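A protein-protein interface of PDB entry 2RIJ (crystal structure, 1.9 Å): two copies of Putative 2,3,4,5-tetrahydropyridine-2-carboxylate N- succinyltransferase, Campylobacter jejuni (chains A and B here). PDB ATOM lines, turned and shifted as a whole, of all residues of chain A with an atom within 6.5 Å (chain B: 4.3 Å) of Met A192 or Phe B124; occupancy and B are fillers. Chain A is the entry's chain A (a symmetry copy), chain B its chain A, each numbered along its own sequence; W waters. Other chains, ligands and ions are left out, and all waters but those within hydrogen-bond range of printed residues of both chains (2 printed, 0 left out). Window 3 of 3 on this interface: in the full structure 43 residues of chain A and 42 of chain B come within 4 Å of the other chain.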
ATOM      1  N   GLU A 187     -10.152 -15.070   7.345  1.00  0.00           N
ATOM      2  CA  GLU A 187      -9.724 -15.259   8.710  1.00  0.00           C
ATOM      3  C   GLU A 187     -10.809 -15.849   9.618  1.00  0.00           C
ATOM      4  O   GLU A 187     -10.519 -16.725  10.429  1.00  0.00           O
ATOM      5  CB  GLU A 187      -9.198 -13.946   9.314  1.00  0.00           C
ATOM      6  CG  GLU A 187      -8.558 -14.139  10.708  1.00  0.00           C
ATOM      7  CD  GLU A 187      -8.214 -12.826  11.418  1.00  0.00           C
ATOM      8  OE1 GLU A 187      -8.390 -11.764  10.797  1.00  0.00           O
ATOM      9  OE2 GLU A 187      -7.807 -12.884  12.609  1.00  0.00           O
ATOM     10  N   MET A 188     -12.025 -15.299   9.574  1.00  0.00           N
ATOM     11  CA  MET A 188     -13.090 -15.786  10.460  1.00  0.00           C
ATOM     12  C   MET A 188     -13.382 -17.250  10.197  1.00  0.00           C
ATOM     13  O   MET A 188     -13.390 -18.057  11.099  1.00  0.00           O
ATOM     14  CB  MET A 188     -14.375 -15.010  10.234  1.00  0.00           C
ATOM     15  CG  MET A 188     -14.290 -13.613  10.656  1.00  0.00           C
ATOM     16  SD  MET A 188     -16.040 -12.792  10.569  1.00  0.00           S
ATOM     17  CE  MET A 188     -15.492 -11.069  11.174  1.00  0.00           C
ATOM     18  N   ARG A 189     -13.579 -17.566   8.926  1.00  0.00           N
ATOM     19  CA  ARG A 189     -13.885 -18.910   8.499  1.00  0.00           C
ATOM     20  C   ARG A 189     -12.759 -19.860   8.895  1.00  0.00           C
ATOM     21  O   ARG A 189     -13.015 -20.910   9.472  1.00  0.00           O
ATOM     22  CB  ARG A 189     -14.131 -18.908   6.986  1.00  0.00           C
ATOM     23  CG  ARG A 189     -14.267 -20.254   6.359  1.00  0.00           C
ATOM     24  CD  ARG A 189     -14.499 -20.138   4.842  1.00  0.00           C
ATOM     25  NE  ARG A 189     -13.314 -19.822   4.032  1.00  0.00           N
ATOM     26  CZ  ARG A 189     -12.305 -20.669   3.815  1.00  0.00           C
ATOM     27  NH1 ARG A 189     -12.300 -21.880   4.378  1.00  0.00           N
ATOM     28  NH2 ARG A 189     -11.277 -20.309   3.044  1.00  0.00           N
ATOM     29  N   LEU A 190     -11.515 -19.494   8.602  1.00  0.00           N
ATOM     30  CA  LEU A 190     -10.387 -20.369   8.871  1.00  0.00           C
ATOM     31  C   LEU A 190     -10.115 -20.562  10.376  1.00  0.00           C
ATOM     32  O   LEU A 190      -9.901 -21.685  10.861  1.00  0.00           O
ATOM     33  CB  LEU A 190      -9.129 -19.853   8.140  1.00  0.00           C
ATOM     34  CG  LEU A 190      -9.102 -19.933   6.597  1.00  0.00           C
ATOM     35  CD1 LEU A 190      -7.874 -19.279   6.005  1.00  0.00           C
ATOM     36  CD2 LEU A 190      -9.159 -21.375   6.136  1.00  0.00           C
ATOM     37  N   LYS A 191     -10.121 -19.488  11.143  1.00  0.00           N
ATOM     38  CA  LYS A 191      -9.887 -19.642  12.577  1.00  0.00           C
ATOM     39  C   LYS A 191     -11.024 -20.383  13.284  1.00  0.00           C
ATOM     40  O   LYS A 191     -10.783 -21.166  14.172  1.00  0.00           O
ATOM     41  CB  LYS A 191      -9.664 -18.321  13.264  1.00  0.00           C
ATOM     42  CG  LYS A 191      -8.355 -17.673  12.911  1.00  0.00           C
ATOM     43  CD  LYS A 191      -8.126 -16.483  13.765  1.00  0.00           C
ATOM     44  CE  LYS A 191      -6.688 -16.033  13.756  1.00  0.00           C
ATOM     45  NZ  LYS A 191      -6.578 -14.732  14.462  1.00  0.00           N
ATOM     46  N   MET A 192     -12.265 -20.105  12.925  1.00  0.00           N
ATOM     47  CA  MET A 192     -13.408 -20.711  13.658  1.00  0.00           C
ATOM     48  C   MET A 192     -13.557 -22.180  13.302  1.00  0.00           C
ATOM     49  O   MET A 192     -13.972 -22.977  14.136  1.00  0.00           O
ATOM     50  CB  MET A 192     -14.707 -19.965  13.367  1.00  0.00           C
ATOM     51  CG  MET A 192     -14.733 -18.570  13.934  1.00  0.00           C
ATOM     52  SD  MET A 192     -14.377 -18.434  15.913  1.00  0.00           S
ATOM     53  CE  MET A 192     -12.484 -17.884  15.951  1.00  0.00           C
ATOM     54  N   SER A 193     -13.197 -22.509  12.072  1.00  0.00           N
ATOM     55  CA  SER A 193     -13.210 -23.895  11.582  1.00  0.00           C
ATOM     56  C   SER A 193     -11.931 -24.621  11.937  1.00  0.00           C
ATOM     57  O   SER A 193     -11.773 -25.763  11.586  1.00  0.00           O
ATOM     58  CB  SER A 193     -13.427 -23.928  10.070  1.00  0.00           C
ATOM     59  OG  SER A 193     -12.275 -23.557   9.393  1.00  0.00           O
ATOM     60  N   ASN A 194     -11.016 -23.939  12.613  1.00  0.00           N
ATOM     61  CA  ASN A 194      -9.720 -24.464  12.980  1.00  0.00           C
ATOM     62  C   ASN A 194      -8.876 -24.962  11.780  1.00  0.00           C
ATOM     63  O   ASN A 194      -8.303 -26.059  11.789  1.00  0.00           O
ATOM     64  CB  ASN A 194      -9.883 -25.546  14.025  1.00  0.00           C
ATOM     65  CG  ASN A 194      -8.577 -25.890  14.713  1.00  0.00           C
ATOM     66  OD1 ASN A 194      -7.580 -25.224  14.520  1.00  0.00           O
ATOM     67  ND2 ASN A 194      -8.590 -26.920  15.543  1.00  0.00           N
ATOM     68  N   GLN A 195      -8.782 -24.131  10.756  1.00  0.00           N
ATOM     69  CA  GLN A 195      -8.042 -24.427   9.550  1.00  0.00           C
ATOM     70  C   GLN A 195      -7.106 -23.247   9.221  1.00  0.00           C
ATOM     71  O   GLN A 195      -6.797 -23.031   8.080  1.00  0.00           O
ATOM     72  CB  GLN A 195      -9.020 -24.604   8.387  1.00  0.00           C
ATOM     73  CG  GLN A 195     -10.035 -25.751   8.518  1.00  0.00           C
ATOM     74  CD  GLN A 195     -10.959 -25.823   7.312  1.00  0.00           C
ATOM     75  OE1 GLN A 195     -10.737 -26.618   6.406  1.00  0.00           O
ATOM     76  NE2 GLN A 195     -11.975 -24.958   7.276  1.00  0.00           N
ATOM     77  N   ILE B  30     -15.220 -13.573  20.658  1.00  0.00           N
ATOM     78  CA  ILE B  30     -15.440 -14.998  20.760  1.00  0.00           C
ATOM     79  C   ILE B  30     -14.173 -15.750  20.319  1.00  0.00           C
ATOM     80  O   ILE B  30     -13.674 -15.570  19.194  1.00  0.00           O
ATOM     81  CB  ILE B  30     -16.674 -15.450  19.918  1.00  0.00           C
ATOM     82  CG1 ILE B  30     -17.950 -14.800  20.415  1.00  0.00           C
ATOM     83  CG2 ILE B  30     -16.834 -16.986  19.932  1.00  0.00           C
ATOM     84  CD1 ILE B  30     -19.173 -15.023  19.438  1.00  0.00           C
ATOM     85  N   ALA B  31     -13.697 -16.615  21.194  1.00  0.00           N
ATOM     86  CA  ALA B  31     -12.531 -17.428  20.959  1.00  0.00           C
ATOM     87  C   ALA B  31     -12.851 -18.888  20.666  1.00  0.00           C
ATOM     88  O   ALA B  31     -13.745 -19.459  21.268  1.00  0.00           O
ATOM     89  CB  ALA B  31     -11.624 -17.366  22.177  1.00  0.00           C
ATOM     90  N   ARG B  32     -12.106 -19.498  19.743  1.00  0.00           N
ATOM     91  CA  ARG B  32     -12.052 -20.939  19.615  1.00  0.00           C
ATOM     92  C   ARG B  32     -10.945 -21.396  20.538  1.00  0.00           C
ATOM     93  O   ARG B  32      -9.807 -20.883  20.477  1.00  0.00           O
ATOM     94  CB  ARG B  32     -11.750 -21.365  18.176  1.00  0.00           C
ATOM     95  CG  ARG B  32     -11.730 -22.851  17.977  1.00  0.00           C
ATOM     96  CD  ARG B  32     -11.223 -23.292  16.568  1.00  0.00           C
ATOM     97  NE  ARG B  32      -9.901 -22.727  16.277  1.00  0.00           N
ATOM     98  CZ  ARG B  32      -8.760 -23.137  16.829  1.00  0.00           C
ATOM     99  NH1 ARG B  32      -8.719 -24.108  17.709  1.00  0.00           N
ATOM    100  NH2 ARG B  32      -7.624 -22.525  16.503  1.00  0.00           N
ATOM    101  N   SER B  47      -8.094 -18.488  20.233  1.00  0.00           N
ATOM    102  CA  SER B  47      -7.929 -17.783  18.963  1.00  0.00           C
ATOM    103  C   SER B  47      -9.196 -16.965  18.662  1.00  0.00           C
ATOM    104  O   SER B  47     -10.314 -17.480  18.771  1.00  0.00           O
ATOM    105  CB  SER B  47      -7.622 -18.772  17.827  1.00  0.00           C
ATOM    106  OG  SER B  47      -6.481 -19.586  18.136  1.00  0.00           O
ATOM    107  N   ALA B  49     -11.004 -14.223  15.744  1.00  0.00           N
ATOM    108  CA  ALA B  49     -10.938 -13.650  14.411  1.00  0.00           C
ATOM    109  C   ALA B  49     -11.426 -12.214  14.377  1.00  0.00           C
ATOM    110  O   ALA B  49     -11.306 -11.561  13.340  1.00  0.00           O
ATOM    111  CB  ALA B  49     -11.752 -14.505  13.416  1.00  0.00           C
ATOM    112  N   THR B  84     -18.514 -20.448  28.035  1.00  0.00           N
ATOM    113  CA  THR B  84     -18.646 -21.350  26.878  1.00  0.00           C
ATOM    114  C   THR B  84     -19.963 -21.109  26.207  1.00  0.00           C
ATOM    115  O   THR B  84     -20.989 -20.995  26.879  1.00  0.00           O
ATOM    116  CB  THR B  84     -18.596 -22.844  27.347  1.00  0.00           C
ATOM    117  OG1 THR B  84     -17.309 -23.108  27.872  1.00  0.00           O
ATOM    118  CG2 THR B  84     -18.891 -23.839  26.211  1.00  0.00           C
ATOM    119  N   LEU B  85     -19.932 -21.031  24.880  1.00  0.00           N
ATOM    120  CA  LEU B  85     -21.127 -20.886  24.065  1.00  0.00           C
ATOM    121  C   LEU B  85     -21.760 -22.253  23.761  1.00  0.00           C
ATOM    122  O   LEU B  85     -21.070 -23.226  23.424  1.00  0.00           O
ATOM    123  CB  LEU B  85     -20.806 -20.178  22.742  1.00  0.00           C
ATOM    124  CG  LEU B  85     -20.495 -18.696  22.888  1.00  0.00           C
ATOM    125  CD1 LEU B  85     -19.615 -18.281  21.716  1.00  0.00           C
ATOM    126  CD2 LEU B  85     -21.844 -17.872  22.969  1.00  0.00           C
ATOM    127  N   LEU B 111     -19.620 -13.586  12.009  1.00  0.00           N
ATOM    128  CA  LEU B 111     -18.866 -14.525  12.821  1.00  0.00           C
ATOM    129  C   LEU B 111     -19.822 -15.556  13.437  1.00  0.00           C
ATOM    130  O   LEU B 111     -19.542 -16.748  13.423  1.00  0.00           O
ATOM    131  CB  LEU B 111     -18.065 -13.785  13.926  1.00  0.00           C
ATOM    132  CG  LEU B 111     -17.211 -14.740  14.802  1.00  0.00           C
ATOM    133  CD1 LEU B 111     -16.003 -15.242  13.979  1.00  0.00           C
ATOM    134  CD2 LEU B 111     -16.772 -14.052  16.081  1.00  0.00           C
ATOM    135  N   ILE B 114     -20.922 -18.145  11.070  1.00  0.00           N
ATOM    136  CA  ILE B 114     -19.826 -19.112  10.872  1.00  0.00           C
ATOM    137  C   ILE B 114     -19.727 -20.095  12.034  1.00  0.00           C
ATOM    138  O   ILE B 114     -19.612 -21.284  11.826  1.00  0.00           O
ATOM    139  CB  ILE B 114     -18.455 -18.399  10.640  1.00  0.00           C
ATOM    140  CG1 ILE B 114     -18.397 -17.804   9.233  1.00  0.00           C
ATOM    141  CG2 ILE B 114     -17.284 -19.392  10.797  1.00  0.00           C
ATOM    142  CD1 ILE B 114     -17.402 -16.631   9.035  1.00  0.00           C
ATOM    143  N   ILE B 115     -19.807 -19.586  13.262  1.00  0.00           N
ATOM    144  CA  ILE B 115     -19.723 -20.435  14.437  1.00  0.00           C
ATOM    145  C   ILE B 115     -20.908 -21.418  14.465  1.00  0.00           C
ATOM    146  O   ILE B 115     -20.722 -22.585  14.772  1.00  0.00           O
ATOM    147  CB  ILE B 115     -19.660 -19.589  15.720  1.00  0.00           C
ATOM    148  CG1 ILE B 115     -18.308 -18.865  15.798  1.00  0.00           C
ATOM    149  CG2 ILE B 115     -19.869 -20.444  16.974  1.00  0.00           C
ATOM    150  CD1 ILE B 115     -18.299 -17.781  16.878  1.00  0.00           C
ATOM    151  N   LYS B 118     -20.139 -24.121  12.111  1.00  0.00           N
ATOM    152  CA  LYS B 118     -19.063 -24.997  12.544  1.00  0.00           C
ATOM    153  C   LYS B 118     -19.155 -25.375  14.019  1.00  0.00           C
ATOM    154  O   LYS B 118     -18.135 -25.729  14.630  1.00  0.00           O
ATOM    155  CB  LYS B 118     -17.703 -24.324  12.300  1.00  0.00           C
ATOM    156  CG  LYS B 118     -17.516 -23.671  10.937  1.00  0.00           C
ATOM    157  CD  LYS B 118     -17.454 -24.719   9.873  1.00  0.00           C
ATOM    158  CE  LYS B 118     -16.956 -24.176   8.554  1.00  0.00           C
ATOM    159  NZ  LYS B 118     -16.934 -25.320   7.598  1.00  0.00           N
ATOM    160  N   PHE B 119     -20.357 -25.305  14.593  1.00  0.00           N
ATOM    161  CA  PHE B 119     -20.515 -25.425  16.036  1.00  0.00           C
ATOM    162  C   PHE B 119     -20.023 -26.756  16.522  1.00  0.00           C
ATOM    163  O   PHE B 119     -20.256 -27.777  15.879  1.00  0.00           O
ATOM    164  CB  PHE B 119     -21.962 -25.233  16.497  1.00  0.00           C
ATOM    165  CG  PHE B 119     -22.086 -25.233  17.980  1.00  0.00           C
ATOM    166  CD1 PHE B 119     -21.743 -24.101  18.703  1.00  0.00           C
ATOM    167  CD2 PHE B 119     -22.453 -26.379  18.661  1.00  0.00           C
ATOM    168  CE1 PHE B 119     -21.781 -24.104  20.078  1.00  0.00           C
ATOM    169  CE2 PHE B 119     -22.496 -26.404  20.035  1.00  0.00           C
ATOM    170  CZ  PHE B 119     -22.168 -25.270  20.748  1.00  0.00           C
ATOM    171  N   LYS B 120     -19.342 -26.736  17.653  1.00  0.00           N
ATOM    172  CA  LYS B 120     -19.052 -27.928  18.416  1.00  0.00           C
ATOM    173  C   LYS B 120     -19.166 -27.530  19.842  1.00  0.00           C
ATOM    174  O   LYS B 120     -18.925 -26.374  20.203  1.00  0.00           O
ATOM    175  CB  LYS B 120     -17.633 -28.443  18.190  1.00  0.00           C
ATOM    176  CG  LYS B 120     -17.270 -28.726  16.767  1.00  0.00           C
ATOM    177  CD  LYS B 120     -15.817 -29.187  16.675  1.00  0.00           C
ATOM    178  CE  LYS B 120     -15.508 -29.791  15.294  1.00  0.00           C
ATOM    179  NZ  LYS B 120     -14.083 -30.264  15.213  1.00  0.00           N
ATOM    180  N   ASP B 122     -18.259 -27.002  23.666  1.00  0.00           N
ATOM    181  CA  ASP B 122     -17.074 -26.586  24.413  1.00  0.00           C
ATOM    182  C   ASP B 122     -15.897 -26.047  23.580  1.00  0.00           C
ATOM    183  O   ASP B 122     -14.775 -25.994  24.055  1.00  0.00           O
ATOM    184  CB  ASP B 122     -16.594 -27.734  25.303  1.00  0.00           C
ATOM    185  CG  ASP B 122     -17.654 -28.183  26.275  1.00  0.00           C
ATOM    186  OD1 ASP B 122     -18.138 -27.340  27.065  1.00  0.00           O
ATOM    187  OD2 ASP B 122     -18.019 -29.371  26.219  1.00  0.00           O
ATOM    188  N   GLU B 123     -16.166 -25.650  22.360  1.00  0.00           N
ATOM    189  CA  GLU B 123     -15.142 -25.245  21.391  1.00  0.00           C
ATOM    190  C   GLU B 123     -14.995 -23.714  21.396  1.00  0.00           C
ATOM    191  O   GLU B 123     -13.915 -23.179  21.147  1.00  0.00           O
ATOM    192  CB  GLU B 123     -15.627 -25.721  20.012  1.00  0.00           C
ATOM    193  CG  GLU B 123     -14.757 -25.391  18.792  1.00  0.00           C
ATOM    194  CD  GLU B 123     -13.658 -26.401  18.545  1.00  0.00           C
ATOM    195  OE1 GLU B 123     -13.518 -27.321  19.367  1.00  0.00           O
ATOM    196  OE2 GLU B 123     -12.957 -26.275  17.525  1.00  0.00           O
ATOM    197  N   PHE B 124     -16.109 -23.012  21.631  1.00  0.00           N
ATOM    198  CA  PHE B 124     -16.173 -21.577  21.531  1.00  0.00           C
ATOM    199  C   PHE B 124     -16.611 -20.946  22.843  1.00  0.00           C
ATOM    200  O   PHE B 124     -17.459 -21.486  23.577  1.00  0.00           O
ATOM    201  CB  PHE B 124     -17.126 -21.166  20.413  1.00  0.00           C
ATOM    202  CG  PHE B 124     -16.807 -21.763  19.088  1.00  0.00           C
ATOM    203  CD1 PHE B 124     -15.853 -21.202  18.275  1.00  0.00           C
ATOM    204  CD2 PHE B 124     -17.521 -22.861  18.617  1.00  0.00           C
ATOM    205  CE1 PHE B 124     -15.543 -21.759  17.011  1.00  0.00           C
ATOM    206  CE2 PHE B 124     -17.233 -23.424  17.362  1.00  0.00           C
ATOM    207  CZ  PHE B 124     -16.261 -22.869  16.555  1.00  0.00           C
ATOM    208  N   SER B 125     -16.012 -19.802  23.146  1.00  0.00           N
ATOM    209  CA  SER B 125     -16.274 -19.094  24.404  1.00  0.00           C
ATOM    210  C   SER B 125     -16.331 -17.594  24.169  1.00  0.00           C
ATOM    211  O   SER B 125     -15.500 -17.020  23.457  1.00  0.00           O
ATOM    212  CB  SER B 125     -15.197 -19.379  25.456  1.00  0.00           C
ATOM    213  OG  SER B 125     -15.289 -20.689  25.993  1.00  0.00           O
HETATM  214  O   HOH W   1     -13.619 -25.585  15.153  1.00  0.00           O
HETATM  215  O   HOH W   2     -11.586 -10.834  10.887  1.00  0.00           O
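NH2 of Arg B32 sits close to OD1 of Asn A194 (3.3 Å). The backbone carbonyl oxygen (O) of Lys A191 lies within hydrogen-bond range of the guanidinium group (NE) of Arg B32, 2.8 Å away.
The side-chain hydroxyl (OG) of Ser A193 is in hydrogen-bond range of the side-chain amide nitrogen (NE2) of Gln A195. The backbone carbonyl oxygen (O) of Leu A190 sits at hydrogen-bond distance from the side-chain hydroxyl (OG) of Ser A193 (3.4 Å). The backbone carbonyl oxygen of Arg A189 lies within hydrogen-bond range of the side-chain hydroxyl of Ser A193 (2.7 Å). N of Leu B85 lies within hydrogen-bond range of O of Phe B124, 2.8 Å away. The backbone NH of Arg B32 lies within hydrogen-bond range of the backbone carbonyl oxygen of Ser B47 (2.9 Å). NZ of Lys A191 is in salt-bridge range of OE2 of Glu A187 (2.9 Å).
No position is printed for both chains. Of the 15 pairs that touch across the chains among the printed residues, none has its exchanged pair printed and touching as well.
Hydrophobic or aromatic side chains of chain A within 4 Å of the printed part of chain B: Met A188 and Met A192. Printed residues of chain B that touch a printed residue of chain A: Arg B32, Ser B47, Ala B49, Leu B111, Ile B114, Ile B115, Lys B118 and Phe B124. Hydrophobic or aromatic side chains of chain B that line the printed part of chain A: Ala B49, Leu B111, Ile B114, Ile B115 and Phe B124. Among the printed residues, no Asp or Glu carboxylate lies within 4 Å of a Lys or Arg side-chain nitrogen of the other chain.
Water W1 bridges OE2 of Glu B123 and O of Met A192. Water W2 lies within hydrogen-bond range of O of Ala B49 (2.6 Å) and OE1 of Glu A187 (3.3 Å).
Among the printed residues, merely in contact across the chains: Glu A187 with Ala B49 (3.7 Å), Met A188 with Ala B49 (3.5 Å), Met A188 with Leu B111 (3.9 Å), Met A188 with Ile B114 (3.6 Å), Arg A189 with Ile B114 (3.9 Å), Met A192 with Arg B32 (3.7 Å), Met A192 with Ser B47 (3.6 Å), Met A192 with Ala B49 (3.95 Å), Met A192 with Leu B111 (3.6 Å), Met A192 with Ile B114 (3.7 Å), Met A192 with Ile B115 (3.96 Å), Met A192 with Phe B124 (3.3 Å) and Ser A193 with Lys B118 (3.8 Å).
Phe B124 touches one residue of chain A. Of the printed residues of chain A, Ser B47 touches Met A192. Of the printed residues of chain A, Arg B32 touches Lys A191, Met A192 and Asn A194. Ser B125 touches none of the printed residues of chain A. The nearest printed residue of chain B that does not touch Met A188 is Ile B115 (6.8 Å).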
